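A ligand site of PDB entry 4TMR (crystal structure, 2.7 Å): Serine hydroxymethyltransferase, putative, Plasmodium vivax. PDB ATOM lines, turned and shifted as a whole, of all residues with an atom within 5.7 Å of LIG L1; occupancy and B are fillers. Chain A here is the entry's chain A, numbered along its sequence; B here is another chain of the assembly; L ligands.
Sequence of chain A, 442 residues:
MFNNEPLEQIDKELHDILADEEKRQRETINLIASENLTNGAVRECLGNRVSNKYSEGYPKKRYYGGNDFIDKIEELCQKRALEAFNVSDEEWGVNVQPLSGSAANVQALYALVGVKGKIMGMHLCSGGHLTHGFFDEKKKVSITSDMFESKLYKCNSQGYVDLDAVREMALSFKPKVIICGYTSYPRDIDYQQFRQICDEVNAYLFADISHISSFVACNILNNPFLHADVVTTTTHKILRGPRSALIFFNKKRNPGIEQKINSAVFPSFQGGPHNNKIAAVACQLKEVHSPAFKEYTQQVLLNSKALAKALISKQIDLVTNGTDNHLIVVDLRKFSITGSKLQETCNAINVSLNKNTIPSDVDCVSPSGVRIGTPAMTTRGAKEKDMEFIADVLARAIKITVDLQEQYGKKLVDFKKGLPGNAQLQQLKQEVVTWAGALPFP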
ATOM      1  N   HIS A 123     -14.057  28.251   3.086  1.00  0.00           N
ATOM      2  CA  HIS A 123     -14.822  27.424   2.171  1.00  0.00           C
ATOM      3  C   HIS A 123     -14.458  27.686   0.718  1.00  0.00           C
ATOM      4  O   HIS A 123     -14.113  28.810   0.315  1.00  0.00           O
ATOM      5  CB  HIS A 123     -16.282  27.743   2.411  1.00  0.00           C
ATOM      6  CG  HIS A 123     -17.227  26.681   1.926  1.00  0.00           C
ATOM      7  ND1 HIS A 123     -17.502  26.490   0.619  1.00  0.00           N
ATOM      8  CD2 HIS A 123     -18.014  25.759   2.622  1.00  0.00           C
ATOM      9  CE1 HIS A 123     -18.386  25.490   0.476  1.00  0.00           C
ATOM     10  NE2 HIS A 123     -18.701  25.038   1.718  1.00  0.00           N
ATOM     11  N   LEU A 124     -14.543  26.630  -0.090  1.00  0.00           N
ATOM     12  CA  LEU A 124     -14.213  26.712  -1.509  1.00  0.00           C
ATOM     13  C   LEU A 124     -15.001  27.800  -2.222  1.00  0.00           C
ATOM     14  O   LEU A 124     -14.435  28.655  -2.880  1.00  0.00           O
ATOM     15  CB  LEU A 124     -14.486  25.368  -2.163  1.00  0.00           C
ATOM     16  CG  LEU A 124     -13.971  25.136  -3.574  1.00  0.00           C
ATOM     17  CD1 LEU A 124     -12.552  24.588  -3.544  1.00  0.00           C
ATOM     18  CD2 LEU A 124     -14.927  24.187  -4.277  1.00  0.00           C
ATOM     19  N   CYS A 125     -16.328  27.733  -2.067  1.00  0.00           N
ATOM     20  CA  CYS A 125     -17.285  28.693  -2.637  1.00  0.00           C
ATOM     21  C   CYS A 125     -16.996  30.136  -2.270  1.00  0.00           C
ATOM     22  O   CYS A 125     -17.482  31.039  -2.929  1.00  0.00           O
ATOM     23  CB  CYS A 125     -18.709  28.348  -2.182  1.00  0.00           C
ATOM     24  SG  CYS A 125     -19.581  27.100  -3.170  1.00  0.00           S
ATOM     25  N   GLY A 127     -13.748  31.305  -1.784  1.00  0.00           N
ATOM     26  CA  GLY A 127     -12.403  31.668  -2.245  1.00  0.00           C
ATOM     27  C   GLY A 127     -11.283  30.840  -1.642  1.00  0.00           C
ATOM     28  O   GLY A 127     -10.118  31.025  -1.997  1.00  0.00           O
ATOM     29  N   GLY A 128     -11.634  29.911  -0.747  1.00  0.00           N
ATOM     30  CA  GLY A 128     -10.672  28.967  -0.173  1.00  0.00           C
ATOM     31  C   GLY A 128     -10.277  27.842  -1.122  1.00  0.00           C
ATOM     32  O   GLY A 128     -10.945  27.594  -2.119  1.00  0.00           O
ATOM     33  N   HIS A 129      -9.169  27.167  -0.815  1.00  0.00           N
ATOM     34  CA  HIS A 129      -8.684  26.062  -1.632  1.00  0.00           C
ATOM     35  C   HIS A 129      -9.220  24.776  -1.125  1.00  0.00           C
ATOM     36  O   HIS A 129      -9.689  24.684   0.020  1.00  0.00           O
ATOM     37  CB  HIS A 129      -7.158  26.019  -1.631  1.00  0.00           C
ATOM     38  CG  HIS A 129      -6.580  25.156  -2.726  1.00  0.00           C
ATOM     39  ND1 HIS A 129      -5.919  24.005  -2.469  1.00  0.00           N
ATOM     40  CD2 HIS A 129      -6.626  25.279  -4.121  1.00  0.00           C
ATOM     41  CE1 HIS A 129      -5.539  23.447  -3.640  1.00  0.00           C
ATOM     42  NE2 HIS A 129      -5.981  24.228  -4.641  1.00  0.00           N
ATOM     43  N   LEU A 130      -9.160  23.746  -1.970  1.00  0.00           N
ATOM     44  CA  LEU A 130      -9.561  22.392  -1.597  1.00  0.00           C
ATOM     45  C   LEU A 130      -8.801  21.892  -0.384  1.00  0.00           C
ATOM     46  O   LEU A 130      -9.392  21.350   0.539  1.00  0.00           O
ATOM     47  CB  LEU A 130      -9.342  21.446  -2.773  1.00  0.00           C
ATOM     48  CG  LEU A 130     -10.114  21.807  -4.037  1.00  0.00           C
ATOM     49  CD1 LEU A 130      -9.349  21.393  -5.284  1.00  0.00           C
ATOM     50  CD2 LEU A 130     -11.507  21.208  -3.996  1.00  0.00           C
ATOM     51  N   PHE A 134     -11.760  21.260   2.590  1.00  0.00           N
ATOM     52  CA  PHE A 134     -13.027  21.286   1.874  1.00  0.00           C
ATOM     53  C   PHE A 134     -13.813  19.974   1.936  1.00  0.00           C
ATOM     54  O   PHE A 134     -13.271  18.900   1.625  1.00  0.00           O
ATOM     55  CB  PHE A 134     -12.859  21.703   0.413  1.00  0.00           C
ATOM     56  CG  PHE A 134     -14.164  21.784  -0.333  1.00  0.00           C
ATOM     57  CD1 PHE A 134     -15.172  22.671   0.067  1.00  0.00           C
ATOM     58  CD2 PHE A 134     -14.412  20.949  -1.418  1.00  0.00           C
ATOM     59  CE1 PHE A 134     -16.382  22.733  -0.590  1.00  0.00           C
ATOM     60  CE2 PHE A 134     -15.630  21.016  -2.085  1.00  0.00           C
ATOM     61  CZ  PHE A 134     -16.612  21.911  -1.673  1.00  0.00           C
ATOM     62  N   ASP A 136     -18.148  18.661   1.010  1.00  0.00           N
ATOM     63  CA  ASP A 136     -19.576  18.786   0.708  1.00  0.00           C
ATOM     64  C   ASP A 136     -20.247  17.976   1.824  1.00  0.00           C
ATOM     65  O   ASP A 136     -19.557  17.320   2.598  1.00  0.00           O
ATOM     66  CB  ASP A 136     -19.858  18.138  -0.646  1.00  0.00           C
ATOM     67  CG  ASP A 136     -21.091  18.699  -1.338  1.00  0.00           C
ATOM     68  OD1 ASP A 136     -20.973  19.765  -1.997  1.00  0.00           O
ATOM     69  OD2 ASP A 136     -22.180  18.065  -1.250  1.00  0.00           O
ATOM     70  N   VAL A 141     -14.481  15.678   0.249  1.00  0.00           N
ATOM     71  CA  VAL A 141     -13.869  15.956  -1.017  1.00  0.00           C
ATOM     72  C   VAL A 141     -12.348  16.036  -0.990  1.00  0.00           C
ATOM     73  O   VAL A 141     -11.702  15.595  -1.881  1.00  0.00           O
ATOM     74  CB  VAL A 141     -14.483  17.222  -1.606  1.00  0.00           C
ATOM     75  CG1 VAL A 141     -13.804  17.635  -2.869  1.00  0.00           C
ATOM     76  CG2 VAL A 141     -15.931  16.993  -1.844  1.00  0.00           C
ATOM     77  N   THR A 183      -7.556  31.020  -2.682  1.00  0.00           N
ATOM     78  CA  THR A 183      -7.349  30.730  -4.088  1.00  0.00           C
ATOM     79  C   THR A 183      -7.997  31.740  -5.042  1.00  0.00           C
ATOM     80  O   THR A 183      -7.409  32.108  -6.048  1.00  0.00           O
ATOM     81  CB  THR A 183      -7.623  29.250  -4.448  1.00  0.00           C
ATOM     82  OG1 THR A 183      -8.741  29.101  -5.333  1.00  0.00           O
ATOM     83  CG2 THR A 183      -7.861  28.467  -3.229  1.00  0.00           C
ATOM     84  N   SER A 184      -9.191  32.223  -4.721  1.00  0.00           N
ATOM     85  CA  SER A 184      -9.810  33.301  -5.497  1.00  0.00           C
ATOM     86  C   SER A 184     -10.306  34.430  -4.620  1.00  0.00           C
ATOM     87  O   SER A 184     -11.490  34.673  -4.495  1.00  0.00           O
ATOM     88  CB  SER A 184     -10.946  32.757  -6.370  1.00  0.00           C
ATOM     89  OG  SER A 184     -11.767  31.878  -5.634  1.00  0.00           O
ATOM     90  N   ASN A 354     -11.599  30.926 -15.988  1.00  0.00           N
ATOM     91  CA  ASN A 354     -12.307  29.832 -15.334  1.00  0.00           C
ATOM     92  C   ASN A 354     -13.535  30.347 -14.667  1.00  0.00           C
ATOM     93  O   ASN A 354     -13.591  31.497 -14.263  1.00  0.00           O
ATOM     94  CB  ASN A 354     -11.409  29.082 -14.337  1.00  0.00           C
ATOM     95  CG  ASN A 354     -11.004  29.922 -13.134  1.00  0.00           C
ATOM     96  OD1 ASN A 354     -10.076  30.742 -13.196  1.00  0.00           O
ATOM     97  ND2 ASN A 354     -11.689  29.710 -12.011  1.00  0.00           N
ATOM     98  N   LYS A 355     -14.540  29.500 -14.587  1.00  0.00           N
ATOM     99  CA  LYS A 355     -15.722  29.801 -13.820  1.00  0.00           C
ATOM    100  C   LYS A 355     -15.348  29.901 -12.326  1.00  0.00           C
ATOM    101  O   LYS A 355     -14.339  29.369 -11.896  1.00  0.00           O
ATOM    102  CB  LYS A 355     -16.778  28.729 -14.044  1.00  0.00           C
ATOM    103  CG  LYS A 355     -16.231  27.319 -14.106  1.00  0.00           C
ATOM    104  CD  LYS A 355     -17.340  26.305 -13.879  1.00  0.00           C
ATOM    105  CE  LYS A 355     -16.761  24.940 -13.574  1.00  0.00           C
ATOM    106  NZ  LYS A 355     -17.794  23.881 -13.732  1.00  0.00           N
ATOM    107  N   ASN A 356     -16.189  30.582 -11.567  1.00  0.00           N
ATOM    108  CA  ASN A 356     -15.928  30.825 -10.165  1.00  0.00           C
ATOM    109  C   ASN A 356     -17.229  31.070  -9.456  1.00  0.00           C
ATOM    110  O   ASN A 356     -18.168  31.595 -10.043  1.00  0.00           O
ATOM    111  CB  ASN A 356     -15.013  32.046 -10.005  1.00  0.00           C
ATOM    112  CG  ASN A 356     -14.170  31.983  -8.748  1.00  0.00           C
ATOM    113  OD1 ASN A 356     -13.041  31.504  -8.771  1.00  0.00           O
ATOM    114  ND2 ASN A 356     -14.713  32.439  -7.652  1.00  0.00           N
ATOM    115  N   THR A 357     -17.291  30.679  -8.194  1.00  0.00           N
ATOM    116  CA  THR A 357     -18.446  30.934  -7.355  1.00  0.00           C
ATOM    117  C   THR A 357     -18.433  32.381  -6.859  1.00  0.00           C
ATOM    118  O   THR A 357     -17.388  33.043  -6.869  1.00  0.00           O
ATOM    119  CB  THR A 357     -18.435  30.008  -6.136  1.00  0.00           C
ATOM    120  OG1 THR A 357     -17.073  29.663  -5.842  1.00  0.00           O
ATOM    121  CG2 THR A 357     -19.183  28.728  -6.431  1.00  0.00           C
ATOM    122  N   CYS A 364     -21.396  24.472  -6.669  1.00  0.00           N
ATOM    123  CA  CYS A 364     -20.210  24.619  -7.539  1.00  0.00           C
ATOM    124  C   CYS A 364     -20.609  24.348  -8.971  1.00  0.00           C
ATOM    125  O   CYS A 364     -19.779  24.357  -9.883  1.00  0.00           O
ATOM    126  CB  CYS A 364     -19.093  23.650  -7.160  1.00  0.00           C
ATOM    127  SG  CYS A 364     -18.889  23.428  -5.386  1.00  0.00           S
ATOM    128  N   VAL A 365     -21.902  24.075  -9.160  1.00  0.00           N
ATOM    129  CA  VAL A 365     -22.475  23.844 -10.471  1.00  0.00           C
ATOM    130  C   VAL A 365     -23.551  24.902 -10.672  1.00  0.00           C
ATOM    131  O   VAL A 365     -24.449  25.108  -9.821  1.00  0.00           O
ATOM    132  CB  VAL A 365     -23.023  22.392 -10.613  1.00  0.00           C
ATOM    133  CG1 VAL A 365     -24.161  22.311 -11.634  1.00  0.00           C
ATOM    134  CG2 VAL A 365     -21.876  21.408 -10.911  1.00  0.00           C
ATOM    135  N   PRO A 367     -22.376  28.083 -11.075  1.00  0.00           N
ATOM    136  CA  PRO A 367     -21.772  29.300 -10.470  1.00  0.00           C
ATOM    137  C   PRO A 367     -21.992  30.569 -11.309  1.00  0.00           C
ATOM    138  O   PRO A 367     -22.063  30.509 -12.551  1.00  0.00           O
ATOM    139  CB  PRO A 367     -20.280  28.954 -10.417  1.00  0.00           C
ATOM    140  CG  PRO A 367     -20.084  27.933 -11.476  1.00  0.00           C
ATOM    141  CD  PRO A 367     -21.333  27.094 -11.408  1.00  0.00           C
ATOM    142  N   ARG A 371     -13.344  34.069 -12.957  1.00  0.00           N
ATOM    143  CA  ARG A 371     -12.220  34.640 -12.286  1.00  0.00           C
ATOM    144  C   ARG A 371     -11.132  34.909 -13.299  1.00  0.00           C
ATOM    145  O   ARG A 371     -10.653  34.005 -13.962  1.00  0.00           O
ATOM    146  CB  ARG A 371     -11.717  33.677 -11.222  1.00  0.00           C
ATOM    147  CG  ARG A 371     -10.569  34.200 -10.379  1.00  0.00           C
ATOM    148  CD  ARG A 371      -9.947  33.064  -9.595  1.00  0.00           C
ATOM    149  NE  ARG A 371      -9.136  32.167 -10.416  1.00  0.00           N
ATOM    150  CZ  ARG A 371      -8.346  31.226  -9.926  1.00  0.00           C
ATOM    151  NH1 ARG A 371      -8.275  31.059  -8.621  1.00  0.00           N
ATOM    152  NH2 ARG A 371      -7.638  30.444 -10.723  1.00  0.00           N
ATOM    153  N   GLU B  56      -6.710  20.948 -13.739  1.00  0.00           N
ATOM    154  CA  GLU B  56      -7.317  20.124 -12.700  1.00  0.00           C
ATOM    155  C   GLU B  56      -8.496  19.378 -13.267  1.00  0.00           C
ATOM    156  O   GLU B  56      -9.353  19.967 -13.919  1.00  0.00           O
ATOM    157  CB  GLU B  56      -7.748  20.969 -11.509  1.00  0.00           C
ATOM    158  CG  GLU B  56      -6.613  21.837 -11.002  1.00  0.00           C
ATOM    159  CD  GLU B  56      -6.966  22.584  -9.758  1.00  0.00           C
ATOM    160  OE1 GLU B  56      -7.146  21.956  -8.714  1.00  0.00           O
ATOM    161  OE2 GLU B  56      -7.066  23.816  -9.813  1.00  0.00           O
ATOM    162  N   TYR B  63     -11.949  21.421 -15.364  1.00  0.00           N
ATOM    163  CA  TYR B  63     -12.672  22.525 -14.775  1.00  0.00           C
ATOM    164  C   TYR B  63     -12.449  23.721 -15.678  1.00  0.00           C
ATOM    165  O   TYR B  63     -13.222  24.678 -15.657  1.00  0.00           O
ATOM    166  CB  TYR B  63     -12.239  22.761 -13.319  1.00  0.00           C
ATOM    167  CG  TYR B  63     -12.848  21.725 -12.384  1.00  0.00           C
ATOM    168  CD1 TYR B  63     -12.306  20.444 -12.281  1.00  0.00           C
ATOM    169  CD2 TYR B  63     -14.007  22.000 -11.659  1.00  0.00           C
ATOM    170  CE1 TYR B  63     -12.883  19.491 -11.459  1.00  0.00           C
ATOM    171  CE2 TYR B  63     -14.597  21.051 -10.833  1.00  0.00           C
ATOM    172  CZ  TYR B  63     -14.029  19.788 -10.732  1.00  0.00           C
ATOM    173  OH  TYR B  63     -14.594  18.819  -9.907  1.00  0.00           O
ATOM    174  N   TYR B  64     -11.412  23.655 -16.503  1.00  0.00           N
ATOM    175  CA  TYR B  64     -11.178  24.711 -17.494  1.00  0.00           C
ATOM    176  C   TYR B  64     -11.369  24.255 -18.934  1.00  0.00           C
ATOM    177  O   TYR B  64     -11.878  23.161 -19.202  1.00  0.00           O
ATOM    178  CB  TYR B  64      -9.789  25.334 -17.324  1.00  0.00           C
ATOM    179  CG  TYR B  64      -9.398  25.648 -15.904  1.00  0.00           C
ATOM    180  CD1 TYR B  64     -10.340  25.634 -14.883  1.00  0.00           C
ATOM    181  CD2 TYR B  64      -8.078  25.992 -15.592  1.00  0.00           C
ATOM    182  CE1 TYR B  64      -9.977  25.935 -13.592  1.00  0.00           C
ATOM    183  CE2 TYR B  64      -7.689  26.301 -14.289  1.00  0.00           C
ATOM    184  CZ  TYR B  64      -8.647  26.273 -13.292  1.00  0.00           C
ATOM    185  OH  TYR B  64      -8.287  26.575 -11.979  1.00  0.00           O
ATOM    186  N   PHE B 266      -7.032  13.250  -7.648  1.00  0.00           N
ATOM    187  CA  PHE B 266      -7.643  14.562  -7.504  1.00  0.00           C
ATOM    188  C   PHE B 266      -9.124  14.341  -7.399  1.00  0.00           C
ATOM    189  O   PHE B 266      -9.634  13.502  -8.097  1.00  0.00           O
ATOM    190  CB  PHE B 266      -7.325  15.454  -8.704  1.00  0.00           C
ATOM    191  CG  PHE B 266      -8.132  16.739  -8.736  1.00  0.00           C
ATOM    192  CD1 PHE B 266      -9.425  16.780  -9.299  1.00  0.00           C
ATOM    193  CD2 PHE B 266      -7.601  17.916  -8.229  1.00  0.00           C
ATOM    194  CE1 PHE B 266     -10.162  17.953  -9.336  1.00  0.00           C
ATOM    195  CE2 PHE B 266      -8.333  19.082  -8.266  1.00  0.00           C
ATOM    196  CZ  PHE B 266      -9.613  19.106  -8.826  1.00  0.00           C
ATOM    197  N   PRO B 267      -9.826  15.109  -6.555  1.00  0.00           N
ATOM    198  CA  PRO B 267      -9.315  16.178  -5.704  1.00  0.00           C
ATOM    199  C   PRO B 267      -8.990  15.803  -4.260  1.00  0.00           C
ATOM    200  O   PRO B 267      -8.785  16.686  -3.439  1.00  0.00           O
ATOM    201  CB  PRO B 267     -10.452  17.180  -5.707  1.00  0.00           C
ATOM    202  CG  PRO B 267     -11.656  16.296  -5.767  1.00  0.00           C
ATOM    203  CD  PRO B 267     -11.290  15.157  -6.661  1.00  0.00           C
HETATM  204  O1  LIG L   1     -17.112  19.159  -5.772  1.00  0.00           O
HETATM  205  C1  LIG L   1     -15.928  18.986  -6.038  1.00  0.00           C
HETATM  206  O2  LIG L   1     -15.290  17.717  -5.802  1.00  0.00           O
HETATM  207  C2  LIG L   1     -16.243  16.806  -5.248  1.00  0.00           C
HETATM  208  C3  LIG L   1     -15.084  20.051  -6.611  1.00  0.00           C
HETATM  209  C4  LIG L   1     -13.751  20.045  -6.983  1.00  0.00           C
HETATM  210  C5  LIG L   1     -13.337  21.265  -7.512  1.00  0.00           C
HETATM  211  S1  LIG L   1     -15.817  21.575  -6.937  1.00  0.00           S
HETATM  212  C6  LIG L   1     -14.340  22.225  -7.537  1.00  0.00           C
HETATM  213  C7  LIG L   1     -14.329  23.619  -8.023  1.00  0.00           C
HETATM  214  C8  LIG L   1     -15.409  24.130  -8.708  1.00  0.00           C
HETATM  215  C9  LIG L   1     -15.350  25.435  -9.189  1.00  0.00           C
HETATM  216  C10 LIG L   1     -16.370  25.927  -9.776  1.00  0.00           C
HETATM  217  N1  LIG L   1     -17.281  26.379 -10.326  1.00  0.00           N
HETATM  218  C11 LIG L   1     -14.235  26.224  -8.988  1.00  0.00           C
HETATM  219  C12 LIG L   1     -13.194  24.383  -7.841  1.00  0.00           C
HETATM  220  C13 LIG L   1     -13.127  25.694  -8.325  1.00  0.00           C
HETATM  221  C14 LIG L   1     -11.908  26.539  -8.073  1.00  0.00           C
HETATM  222  C15 LIG L   1     -11.468  27.394  -9.283  1.00  0.00           C
HETATM  223  C16 LIG L   1     -11.091  26.591 -10.526  1.00  0.00           C
HETATM  224  C17 LIG L   1     -10.331  28.354  -8.936  1.00  0.00           C
HETATM  225  C18 LIG L   1     -12.381  27.478  -6.977  1.00  0.00           C
HETATM  226  C19 LIG L   1     -13.404  28.204  -7.172  1.00  0.00           C
HETATM  227  N2  LIG L   1     -14.330  28.868  -7.330  1.00  0.00           N
HETATM  228  C20 LIG L   1     -11.746  27.650  -5.805  1.00  0.00           C
HETATM  229  N3  LIG L   1     -12.091  28.646  -4.980  1.00  0.00           N
HETATM  230  C21 LIG L   1     -10.804  25.694  -7.525  1.00  0.00           C
HETATM  231  C22 LIG L   1     -10.028  24.539  -8.047  1.00  0.00           C
HETATM  232  C23 LIG L   1     -10.169  23.857  -9.395  1.00  0.00           C
HETATM  233  N4  LIG L   1      -9.151  24.164  -7.090  1.00  0.00           N
HETATM  234  N5  LIG L   1      -9.260  24.952  -5.925  1.00  0.00           N
HETATM  235  C24 LIG L   1     -10.219  25.838  -6.200  1.00  0.00           C
HETATM  236  O3  LIG L   1     -10.656  26.817  -5.377  1.00  0.00           O
HETATM  237  N1  LG2 L   2      -2.989  26.584  -2.622  1.00  0.00           N
HETATM  238  C1  LG2 L   2      -3.780  27.608  -3.053  1.00  0.00           C
HETATM  239  C2  LG2 L   2      -4.277  28.660  -2.096  1.00  0.00           C
HETATM  240  C3  LG2 L   2      -4.136  27.677  -4.389  1.00  0.00           C
HETATM  241  O1  LG2 L   2      -4.930  28.667  -4.873  1.00  0.00           O
HETATM  242  C4  LG2 L   2      -3.699  26.714  -5.272  1.00  0.00           C
HETATM  243  C5  LG2 L   2      -4.098  26.778  -6.703  1.00  0.00           C
HETATM  244  C6  LG2 L   2      -2.901  25.679  -4.786  1.00  0.00           C
HETATM  245  C7  LG2 L   2      -2.548  25.632  -3.455  1.00  0.00           C
HETATM  246  C8  LG2 L   2      -2.448  24.678  -5.769  1.00  0.00           C
HETATM  247  O2  LG2 L   2      -1.607  23.553  -5.450  1.00  0.00           O
HETATM  248  P1  LG2 L   2      -1.085  22.704  -6.696  1.00  0.00           P
HETATM  249  O3  LG2 L   2      -1.014  21.324  -6.075  1.00  0.00           O
HETATM  250  O4  LG2 L   2      -2.169  22.846  -7.728  1.00  0.00           O
HETATM  251  O5  LG2 L   2       0.237  23.339  -7.022  1.00  0.00           O
HETATM  252  C9  LG2 L   2      -5.967  27.769  -8.979  1.00  0.00           C
HETATM  253  O6  LG2 L   2      -6.374  27.735 -10.160  1.00  0.00           O
HETATM  254  O7  LG2 L   2      -5.693  28.846  -8.392  1.00  0.00           O
HETATM  255  C10 LG2 L   2      -5.827  26.406  -8.327  1.00  0.00           C
HETATM  256  N2  LG2 L   2      -5.273  26.430  -6.988  1.00  0.00           N
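The side-chain hydroxyl (OG1) of Thr 183 lies within hydrogen-bond range of an oxygen (O3) of LIG L1, 3.0 Å away.
The side-chain carboxylate of Glu 56 of chain B lies within hydrogen-bond range of a nitrogen (N4) of LIG L1.
O of Leu 124 sits at hydrogen-bond distance from N3 of LIG L1 (3.1 Å).
OG1 of Thr 357 sits at hydrogen-bond distance from N2 of LIG L1, at 3.2 Å.
A nitrogen (N3) of LIG L1 is in hydrogen-bond range of the backbone carbonyl oxygen (O) of Gly 128 (3.3 Å).
OD1 of Asn 356 lies close to N2 of LIG L1 (3.3 Å).
OG of Ser 184 sits at hydrogen-bond distance from N3 of LIG L1 (3.3 Å).
An oxygen (O6) of LG2 L2 lies within hydrogen-bond range of the side-chain hydroxyl of Tyr 64 of chain B, 2.9 Å away.
A ring nitrogen (NE2) of His 129 sits at hydrogen-bond distance from a nitrogen (N2) of LG2 L2, 3.3 Å away.
An oxygen (O6) of LG2 L2 is in salt-bridge range of the guanidinium group of Arg 371 (3.0 Å).
The backbone carbonyl oxygen of Thr 183 lies within hydrogen-bond range of the guanidinium group of Arg 371 (2.9 Å).
The backbone NH of Thr 183 is in hydrogen-bond range of the backbone carbonyl oxygen of Gly 127, 2.7 Å away.
O of Glu 56 of chain B is in hydrogen-bond range of N of Tyr 63 of chain B.
O of Cys 125 is in hydrogen-bond range of OG1 of Thr 357 (3.2 Å).
N of Gly 128 lies within hydrogen-bond range of O of His 123 (2.9 Å).
The side-chain amide oxygen (OD1) of Asn 356 lies within hydrogen-bond range of the side-chain hydroxyl (OG) of Ser 184 (3.4 Å).
N of Ser 184 is in hydrogen-bond range of O of Gly 127 (3.1 Å).
N of Arg 371 sits at hydrogen-bond distance from O of Asn 354, 2.9 Å away.
O of Cys 364 sits close to N1 of LIG L1 (3.2 Å).
His 129 touches LIG L1 (CD2 to N5, 3.2 Å).
CD1 of Leu 130 touches N4 of LIG L1, 3.3 Å away.
Val 141 touches LIG L1.
ND2 of Asn 354 touches C16 of LIG L1, 3.5 Å away.
Lys 355 touches LIG L1 (CD to N1, 3.6 Å).
CG of Pro 367 touches N1 of LIG L1, at 3.4 Å.
Arg 371 touches LIG L1 (NH1 to C17, 3.4 Å).
Tyr 63 of chain B touches LIG L1.
OH of Tyr 64 of chain B touches C16 of LIG L1 (3.2 Å).
Pro 267 of chain B touches LIG L1.
Hydrophobic or aromatic side chains that line LIG L1: Leu 124, His 129, Leu 130, Val 141, Pro 367, Tyr 63 of chain B, Tyr 64 of chain B and Pro 267 of chain B.
18 residues have an atom within 4 Å of LIG L1: Leu 124, Gly 128, His 129, Leu 130, Val 141, Thr 183, Ser 184, Asn 354, Lys 355, Asn 356, Thr 357, Cys 364, Pro 367, Arg 371, Glu 56 of chain B, Tyr 63 of chain B, Tyr 64 of chain B and Pro 267 of chain B.
Along chain A the residues within 4 Å of LIG L1 span positions 124 to 371.
The nearest printed residue that does not touch LIG L1 is Gly 127 (4.1 Å).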
